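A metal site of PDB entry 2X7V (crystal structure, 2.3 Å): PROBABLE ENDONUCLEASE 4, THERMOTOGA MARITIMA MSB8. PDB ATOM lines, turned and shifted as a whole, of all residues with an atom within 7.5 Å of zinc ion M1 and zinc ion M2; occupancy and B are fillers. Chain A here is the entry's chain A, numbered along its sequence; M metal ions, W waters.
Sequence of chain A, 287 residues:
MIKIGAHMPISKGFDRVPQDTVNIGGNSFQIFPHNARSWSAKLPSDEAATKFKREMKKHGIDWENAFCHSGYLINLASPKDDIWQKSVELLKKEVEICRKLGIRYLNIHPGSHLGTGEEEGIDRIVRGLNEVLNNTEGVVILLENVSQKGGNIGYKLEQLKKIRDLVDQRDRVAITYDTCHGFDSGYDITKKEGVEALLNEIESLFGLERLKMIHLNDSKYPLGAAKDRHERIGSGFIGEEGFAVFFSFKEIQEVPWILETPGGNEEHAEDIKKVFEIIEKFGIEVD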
ATOM      1  N   GLN A  30     -24.236  37.180 -12.829  1.00  0.00           N
ATOM      2  CA  GLN A  30     -23.461  36.097 -12.263  1.00  0.00           C
ATOM      3  C   GLN A  30     -21.995  36.523 -12.353  1.00  0.00           C
ATOM      4  O   GLN A  30     -21.611  37.243 -13.262  1.00  0.00           O
ATOM      5  CB  GLN A  30     -23.749  34.802 -13.035  1.00  0.00           C
ATOM      6  CG  GLN A  30     -22.765  33.663 -12.803  1.00  0.00           C
ATOM      7  CD  GLN A  30     -23.180  32.398 -13.513  1.00  0.00           C
ATOM      8  OE1 GLN A  30     -24.011  31.629 -13.016  1.00  0.00           O
ATOM      9  NE2 GLN A  30     -22.624  32.172 -14.699  1.00  0.00           N
ATOM     10  N   PHE A  32     -17.696  35.224 -11.215  1.00  0.00           N
ATOM     11  CA  PHE A  32     -16.780  34.323 -10.534  1.00  0.00           C
ATOM     12  C   PHE A  32     -16.416  34.933  -9.174  1.00  0.00           C
ATOM     13  O   PHE A  32     -16.354  36.160  -9.018  1.00  0.00           O
ATOM     14  CB  PHE A  32     -15.513  34.135 -11.372  1.00  0.00           C
ATOM     15  CG  PHE A  32     -15.722  33.313 -12.610  1.00  0.00           C
ATOM     16  CD1 PHE A  32     -16.271  32.049 -12.523  1.00  0.00           C
ATOM     17  CD2 PHE A  32     -15.349  33.787 -13.851  1.00  0.00           C
ATOM     18  CE1 PHE A  32     -16.463  31.268 -13.662  1.00  0.00           C
ATOM     19  CE2 PHE A  32     -15.542  33.029 -15.005  1.00  0.00           C
ATOM     20  CZ  PHE A  32     -16.106  31.763 -14.895  1.00  0.00           C
ATOM     21  N   HIS A  69     -20.482  31.873  -9.537  1.00  0.00           N
ATOM     22  CA  HIS A  69     -20.276  30.631 -10.248  1.00  0.00           C
ATOM     23  C   HIS A  69     -18.891  30.127  -9.906  1.00  0.00           C
ATOM     24  O   HIS A  69     -17.947  30.906  -9.944  1.00  0.00           O
ATOM     25  CB  HIS A  69     -20.405  30.854 -11.758  1.00  0.00           C
ATOM     26  CG  HIS A  69     -20.457  29.598 -12.557  1.00  0.00           C
ATOM     27  ND1 HIS A  69     -19.496  28.611 -12.465  1.00  0.00           N
ATOM     28  CD2 HIS A  69     -21.370  29.148 -13.454  1.00  0.00           C
ATOM     29  CE1 HIS A  69     -19.805  27.612 -13.263  1.00  0.00           C
ATOM     30  NE2 HIS A  69     -20.926  27.919 -13.886  1.00  0.00           N
ATOM     31  N   SER A  70     -18.763  28.859  -9.556  1.00  0.00           N
ATOM     32  CA  SER A  70     -17.452  28.274  -9.270  1.00  0.00           C
ATOM     33  C   SER A  70     -16.558  28.187 -10.502  1.00  0.00           C
ATOM     34  O   SER A  70     -17.038  28.057 -11.623  1.00  0.00           O
ATOM     35  CB  SER A  70     -17.604  26.868  -8.707  1.00  0.00           C
ATOM     36  OG  SER A  70     -18.252  26.924  -7.467  1.00  0.00           O
ATOM     37  N   ASN A 107     -23.207  28.720  -7.694  1.00  0.00           N
ATOM     38  CA  ASN A 107     -23.523  27.744  -8.725  1.00  0.00           C
ATOM     39  C   ASN A 107     -22.311  26.853  -9.046  1.00  0.00           C
ATOM     40  O   ASN A 107     -21.203  27.350  -9.207  1.00  0.00           O
ATOM     41  CB  ASN A 107     -23.976  28.500  -9.985  1.00  0.00           C
ATOM     42  CG  ASN A 107     -24.368  27.585 -11.114  1.00  0.00           C
ATOM     43  OD1 ASN A 107     -25.518  27.154 -11.222  1.00  0.00           O
ATOM     44  ND2 ASN A 107     -23.400  27.252 -11.966  1.00  0.00           N
ATOM     45  N   ILE A 108     -22.531  25.545  -9.127  1.00  0.00           N
ATOM     46  CA  ILE A 108     -21.471  24.606  -9.501  1.00  0.00           C
ATOM     47  C   ILE A 108     -21.989  23.537 -10.462  1.00  0.00           C
ATOM     48  O   ILE A 108     -23.176  23.207 -10.468  1.00  0.00           O
ATOM     49  CB  ILE A 108     -20.857  23.834  -8.297  1.00  0.00           C
ATOM     50  CG1 ILE A 108     -21.863  22.808  -7.748  1.00  0.00           C
ATOM     51  CG2 ILE A 108     -20.430  24.760  -7.204  1.00  0.00           C
ATOM     52  CD1 ILE A 108     -21.318  21.972  -6.586  1.00  0.00           C
ATOM     53  N   HIS A 109     -21.064  23.017 -11.262  1.00  0.00           N
ATOM     54  CA  HIS A 109     -21.273  21.773 -11.986  1.00  0.00           C
ATOM     55  C   HIS A 109     -20.965  20.669 -11.002  1.00  0.00           C
ATOM     56  O   HIS A 109     -19.964  20.736 -10.286  1.00  0.00           O
ATOM     57  CB  HIS A 109     -20.312  21.705 -13.155  1.00  0.00           C
ATOM     58  CG  HIS A 109     -20.541  22.774 -14.184  1.00  0.00           C
ATOM     59  ND1 HIS A 109     -20.061  22.692 -15.470  1.00  0.00           N
ATOM     60  CD2 HIS A 109     -21.239  23.935 -14.113  1.00  0.00           C
ATOM     61  CE1 HIS A 109     -20.439  23.762 -16.147  1.00  0.00           C
ATOM     62  NE2 HIS A 109     -21.157  24.536 -15.343  1.00  0.00           N
ATOM     63  N   GLU A 144     -26.052  22.674 -11.242  1.00  0.00           N
ATOM     64  CA  GLU A 144     -26.395  22.998 -12.605  1.00  0.00           C
ATOM     65  C   GLU A 144     -26.392  21.759 -13.494  1.00  0.00           C
ATOM     66  O   GLU A 144     -25.466  20.958 -13.428  1.00  0.00           O
ATOM     67  CB  GLU A 144     -25.402  24.007 -13.155  1.00  0.00           C
ATOM     68  CG  GLU A 144     -25.753  24.434 -14.567  1.00  0.00           C
ATOM     69  CD  GLU A 144     -24.722  25.366 -15.182  1.00  0.00           C
ATOM     70  OE1 GLU A 144     -23.990  26.060 -14.448  1.00  0.00           O
ATOM     71  OE2 GLU A 144     -24.647  25.401 -16.407  1.00  0.00           O
ATOM     72  N   ASN A 145     -27.402  21.581 -14.325  1.00  0.00           N
ATOM     73  CA  ASN A 145     -27.346  20.502 -15.295  1.00  0.00           C
ATOM     74  C   ASN A 145     -26.206  20.746 -16.296  1.00  0.00           C
ATOM     75  O   ASN A 145     -25.875  21.891 -16.605  1.00  0.00           O
ATOM     76  CB  ASN A 145     -28.686  20.274 -16.009  1.00  0.00           C
ATOM     77  CG  ASN A 145     -29.114  21.448 -16.873  1.00  0.00           C
ATOM     78  OD1 ASN A 145     -29.295  21.319 -18.093  1.00  0.00           O
ATOM     79  ND2 ASN A 145     -29.287  22.608 -16.248  1.00  0.00           N
ATOM     80  N   VAL A 146     -25.585  19.657 -16.753  1.00  0.00           N
ATOM     81  CA  VAL A 146     -24.468  19.758 -17.687  1.00  0.00           C
ATOM     82  C   VAL A 146     -24.704  18.902 -18.938  1.00  0.00           C
ATOM     83  O   VAL A 146     -25.692  18.187 -19.044  1.00  0.00           O
ATOM     84  CB  VAL A 146     -23.133  19.346 -17.014  1.00  0.00           C
ATOM     85  CG1 VAL A 146     -22.760  20.343 -15.927  1.00  0.00           C
ATOM     86  CG2 VAL A 146     -23.234  17.921 -16.445  1.00  0.00           C
ATOM     87  N   THR A 176     -29.907  25.131 -10.823  1.00  0.00           N
ATOM     88  CA  THR A 176     -29.818  26.043 -11.957  1.00  0.00           C
ATOM     89  C   THR A 176     -30.113  25.229 -13.219  1.00  0.00           C
ATOM     90  O   THR A 176     -29.599  24.132 -13.365  1.00  0.00           O
ATOM     91  CB  THR A 176     -28.393  26.627 -12.088  1.00  0.00           C
ATOM     92  OG1 THR A 176     -28.168  27.584 -11.043  1.00  0.00           O
ATOM     93  CG2 THR A 176     -28.188  27.306 -13.461  1.00  0.00           C
ATOM     94  N   TYR A 177     -30.929  25.753 -14.125  1.00  0.00           N
ATOM     95  CA  TYR A 177     -31.167  25.086 -15.397  1.00  0.00           C
ATOM     96  C   TYR A 177     -30.491  25.843 -16.542  1.00  0.00           C
ATOM     97  O   TYR A 177     -30.730  27.042 -16.750  1.00  0.00           O
ATOM     98  CB  TYR A 177     -32.656  24.944 -15.711  1.00  0.00           C
ATOM     99  CG  TYR A 177     -32.877  24.205 -17.001  1.00  0.00           C
ATOM    100  CD1 TYR A 177     -32.709  22.831 -17.067  1.00  0.00           C
ATOM    101  CD2 TYR A 177     -33.226  24.887 -18.172  1.00  0.00           C
ATOM    102  CE1 TYR A 177     -32.879  22.148 -18.252  1.00  0.00           C
ATOM    103  CE2 TYR A 177     -33.425  24.207 -19.351  1.00  0.00           C
ATOM    104  CZ  TYR A 177     -33.242  22.825 -19.390  1.00  0.00           C
ATOM    105  OH  TYR A 177     -33.412  22.130 -20.567  1.00  0.00           O
ATOM    106  N   ASP A 178     -29.636  25.149 -17.283  1.00  0.00           N
ATOM    107  CA  ASP A 178     -28.917  25.757 -18.386  1.00  0.00           C
ATOM    108  C   ASP A 178     -29.578  25.240 -19.648  1.00  0.00           C
ATOM    109  O   ASP A 178     -29.616  24.024 -19.889  1.00  0.00           O
ATOM    110  CB  ASP A 178     -27.425  25.403 -18.345  1.00  0.00           C
ATOM    111  CG  ASP A 178     -26.620  26.036 -19.490  1.00  0.00           C
ATOM    112  OD1 ASP A 178     -25.587  26.675 -19.231  1.00  0.00           O
ATOM    113  OD2 ASP A 178     -27.008  25.900 -20.661  1.00  0.00           O
ATOM    114  N   THR A 179     -30.108  26.152 -20.454  1.00  0.00           N
ATOM    115  CA  THR A 179     -30.887  25.782 -21.630  1.00  0.00           C
ATOM    116  C   THR A 179     -30.062  25.034 -22.668  1.00  0.00           C
ATOM    117  O   THR A 179     -30.563  24.108 -23.299  1.00  0.00           O
ATOM    118  CB  THR A 179     -31.596  27.011 -22.261  1.00  0.00           C
ATOM    119  OG1 THR A 179     -30.623  27.971 -22.640  1.00  0.00           O
ATOM    120  CG2 THR A 179     -32.574  27.645 -21.249  1.00  0.00           C
ATOM    121  N   CYS A 180     -28.804  25.426 -22.839  1.00  0.00           N
ATOM    122  CA  CYS A 180     -27.884  24.766 -23.772  1.00  0.00           C
ATOM    123  C   CYS A 180     -27.508  23.337 -23.328  1.00  0.00           C
ATOM    124  O   CYS A 180     -27.613  22.385 -24.114  1.00  0.00           O
ATOM    125  CB  CYS A 180     -26.628  25.615 -24.022  1.00  0.00           C
ATOM    126  SG  CYS A 180     -25.419  24.767 -25.083  1.00  0.00           S
ATOM    127  N   HIS A 181     -27.107  23.167 -22.068  1.00  0.00           N
ATOM    128  CA  HIS A 181     -26.820  21.822 -21.557  1.00  0.00           C
ATOM    129  C   HIS A 181     -28.058  20.913 -21.615  1.00  0.00           C
ATOM    130  O   HIS A 181     -27.948  19.743 -21.959  1.00  0.00           O
ATOM    131  CB  HIS A 181     -26.281  21.887 -20.129  1.00  0.00           C
ATOM    132  CG  HIS A 181     -25.061  22.743 -19.985  1.00  0.00           C
ATOM    133  ND1 HIS A 181     -24.703  23.331 -18.784  1.00  0.00           N
ATOM    134  CD2 HIS A 181     -24.119  23.100 -20.872  1.00  0.00           C
ATOM    135  CE1 HIS A 181     -23.593  24.013 -18.947  1.00  0.00           C
ATOM    136  NE2 HIS A 181     -23.214  23.903 -20.210  1.00  0.00           N
ATOM    137  N   MET A 213     -32.265  29.823 -10.853  1.00  0.00           N
ATOM    138  CA  MET A 213     -31.584  30.517 -11.940  1.00  0.00           C
ATOM    139  C   MET A 213     -31.652  29.708 -13.203  1.00  0.00           C
ATOM    140  O   MET A 213     -31.508  28.486 -13.179  1.00  0.00           O
ATOM    141  CB  MET A 213     -30.102  30.754 -11.573  1.00  0.00           C
ATOM    142  CG  MET A 213     -29.233  31.159 -12.769  1.00  0.00           C
ATOM    143  SD  MET A 213     -27.635  31.880 -12.332  1.00  0.00           S
ATOM    144  CE  MET A 213     -26.844  30.569 -11.381  1.00  0.00           C
ATOM    145  N   ILE A 214     -31.869  30.380 -14.329  1.00  0.00           N
ATOM    146  CA  ILE A 214     -31.727  29.737 -15.618  1.00  0.00           C
ATOM    147  C   ILE A 214     -30.506  30.321 -16.302  1.00  0.00           C
ATOM    148  O   ILE A 214     -30.290  31.526 -16.274  1.00  0.00           O
ATOM    149  CB  ILE A 214     -32.974  29.942 -16.477  1.00  0.00           C
ATOM    150  CG1 ILE A 214     -34.143  29.121 -15.895  1.00  0.00           C
ATOM    151  CG2 ILE A 214     -32.722  29.500 -17.900  1.00  0.00           C
ATOM    152  CD1 ILE A 214     -35.502  29.688 -16.155  1.00  0.00           C
ATOM    153  N   HIS A 215     -29.654  29.462 -16.869  1.00  0.00           N
ATOM    154  CA  HIS A 215     -28.649  29.969 -17.789  1.00  0.00           C
ATOM    155  C   HIS A 215     -29.235  29.968 -19.184  1.00  0.00           C
ATOM    156  O   HIS A 215     -29.548  28.926 -19.741  1.00  0.00           O
ATOM    157  CB  HIS A 215     -27.354  29.173 -17.741  1.00  0.00           C
ATOM    158  CG  HIS A 215     -26.571  29.375 -16.497  1.00  0.00           C
ATOM    159  ND1 HIS A 215     -25.635  28.472 -16.049  1.00  0.00           N
ATOM    160  CD2 HIS A 215     -26.599  30.378 -15.591  1.00  0.00           C
ATOM    161  CE1 HIS A 215     -25.104  28.922 -14.922  1.00  0.00           C
ATOM    162  NE2 HIS A 215     -25.671  30.073 -14.629  1.00  0.00           N
ATOM    163  N   LEU A 216     -29.367  31.163 -19.747  1.00  0.00           N
ATOM    164  CA  LEU A 216     -30.016  31.345 -21.018  1.00  0.00           C
ATOM    165  C   LEU A 216     -28.958  31.283 -22.080  1.00  0.00           C
ATOM    166  O   LEU A 216     -28.250  32.271 -22.318  1.00  0.00           O
ATOM    167  CB  LEU A 216     -30.700  32.707 -21.043  1.00  0.00           C
ATOM    168  CG  LEU A 216     -31.809  32.827 -22.071  1.00  0.00           C
ATOM    169  CD1 LEU A 216     -32.886  31.792 -21.750  1.00  0.00           C
ATOM    170  CD2 LEU A 216     -32.360  34.271 -22.104  1.00  0.00           C
ATOM    171  N   ASN A 217     -28.827  30.120 -22.707  1.00  0.00           N
ATOM    172  CA  ASN A 217     -27.837  29.914 -23.765  1.00  0.00           C
ATOM    173  C   ASN A 217     -28.496  29.267 -24.993  1.00  0.00           C
ATOM    174  O   ASN A 217     -29.219  28.281 -24.866  1.00  0.00           O
ATOM    175  CB  ASN A 217     -26.686  29.010 -23.276  1.00  0.00           C
ATOM    176  CG  ASN A 217     -25.987  29.569 -22.054  1.00  0.00           C
ATOM    177  OD1 ASN A 217     -25.798  28.871 -21.042  1.00  0.00           O
ATOM    178  ND2 ASN A 217     -25.590  30.836 -22.131  1.00  0.00           N
ATOM    179  N   ASP A 228     -21.854  20.786 -25.687  1.00  0.00           N
ATOM    180  CA  ASP A 228     -21.480  21.855 -24.772  1.00  0.00           C
ATOM    181  C   ASP A 228     -20.803  23.054 -25.459  1.00  0.00           C
ATOM    182  O   ASP A 228     -19.698  23.484 -25.082  1.00  0.00           O
ATOM    183  CB  ASP A 228     -20.599  21.313 -23.653  1.00  0.00           C
ATOM    184  CG  ASP A 228     -20.435  22.294 -22.518  1.00  0.00           C
ATOM    185  OD1 ASP A 228     -19.419  22.202 -21.788  1.00  0.00           O
ATOM    186  OD2 ASP A 228     -21.318  23.176 -22.387  1.00  0.00           O
ATOM    187  N   HIS A 230     -22.001  26.889 -26.344  1.00  0.00           N
ATOM    188  CA  HIS A 230     -23.034  27.918 -26.268  1.00  0.00           C
ATOM    189  C   HIS A 230     -23.065  28.798 -27.510  1.00  0.00           C
ATOM    190  O   HIS A 230     -22.065  28.946 -28.203  1.00  0.00           O
ATOM    191  CB  HIS A 230     -22.783  28.835 -25.080  1.00  0.00           C
ATOM    192  CG  HIS A 230     -22.795  28.134 -23.760  1.00  0.00           C
ATOM    193  ND1 HIS A 230     -22.614  28.814 -22.567  1.00  0.00           N
ATOM    194  CD2 HIS A 230     -22.955  26.835 -23.433  1.00  0.00           C
ATOM    195  CE1 HIS A 230     -22.664  27.951 -21.566  1.00  0.00           C
ATOM    196  NE2 HIS A 230     -22.880  26.748 -22.061  1.00  0.00           N
ATOM    197  N   ILE A 258     -29.927  34.232 -16.933  1.00  0.00           N
ATOM    198  CA  ILE A 258     -28.540  34.660 -16.965  1.00  0.00           C
ATOM    199  C   ILE A 258     -27.876  34.193 -18.276  1.00  0.00           C
ATOM    200  O   ILE A 258     -27.735  32.999 -18.516  1.00  0.00           O
ATOM    201  CB  ILE A 258     -27.765  34.111 -15.713  1.00  0.00           C
ATOM    202  CG1 ILE A 258     -28.419  34.610 -14.418  1.00  0.00           C
ATOM    203  CG2 ILE A 258     -26.276  34.473 -15.758  1.00  0.00           C
ATOM    204  CD1 ILE A 258     -28.306  36.089 -14.218  1.00  0.00           C
ATOM    205  N   GLU A 260     -24.935  33.304 -20.722  1.00  0.00           N
ATOM    206  CA  GLU A 260     -23.534  32.882 -20.730  1.00  0.00           C
ATOM    207  C   GLU A 260     -23.084  32.658 -22.166  1.00  0.00           C
ATOM    208  O   GLU A 260     -22.274  31.796 -22.455  1.00  0.00           O
ATOM    209  CB  GLU A 260     -23.350  31.580 -19.961  1.00  0.00           C
ATOM    210  CG  GLU A 260     -23.746  31.616 -18.503  1.00  0.00           C
ATOM    211  CD  GLU A 260     -23.493  30.276 -17.870  1.00  0.00           C
ATOM    212  OE1 GLU A 260     -24.043  29.290 -18.411  1.00  0.00           O
ATOM    213  OE2 GLU A 260     -22.728  30.186 -16.872  1.00  0.00           O
HETATM  214 ZN    ZN M   1     -22.001  26.557 -15.341  1.00  0.00          ZN
HETATM  215 ZN    ZN M   2     -24.349  27.276 -17.646  1.00  0.00          ZN
HETATM  216 ZN    ZN M   3     -21.689  25.143 -21.095  1.00  0.00          ZN
HETATM  217  O   HOH W   1     -22.172  27.540 -17.367  1.00  0.00           O
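CE1 of His 181 touches zinc ion M2, at 3.6 Å. Five residues have an atom within 4 Å of zinc ion M2: Glu 144, Asp 178, His 181, His 215 and Glu 260.
N of His 181 sits at hydrogen-bond distance from OD2 of Asp 178 (3.1 Å). N of Glu 144 is in hydrogen-bond range of O of Ile 108 (3.0 Å). OD2 of Asp 178 is in hydrogen-bond range of N of Cys 180, 2.9 Å away. ND1 of His 230 sits at hydrogen-bond distance from O of Glu 260. The backbone NH (N) of Glu 260 sits close to the side-chain amide nitrogen (ND2) of Asn 217 (2.9 Å). A ring nitrogen (ND1) of His 181 lies within hydrogen-bond range of the backbone carbonyl oxygen (O) of Asn 145 (2.9 Å). OE1 of Glu 144 sits close to ND2 of Asn 107 (2.8 Å). A ring nitrogen (NE2) of His 69 lies close to the side-chain amide nitrogen (ND2) of Asn 107.
OD1 of Asp 178 binds zinc ion M2, at 2.1 Å. The side-chain carboxylate (OE1) of Glu 260 binds zinc ion M2 (2.2 Å). Water W1 binds zinc ion M2 (2.2 Å). OE2 of Glu 144 is bound to zinc ion M2. Zinc ion M2 is bound by ND1 of His 215, 2.4 Å away. Zinc ion M2 has five donor atoms within binding distance.
Residues that only touch zinc ion M1: Asn 107.
NE2 of His 109 binds zinc ion M1. Zinc ion M1 is bound by OE1 of Glu 144, 2.2 Å away. Water W1 binds zinc ion M1 (2.3 Å). Zinc ion M1 is bound by a ring nitrogen (NE2) of His 69. Zinc ion M1 has four donor atoms within binding distance.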
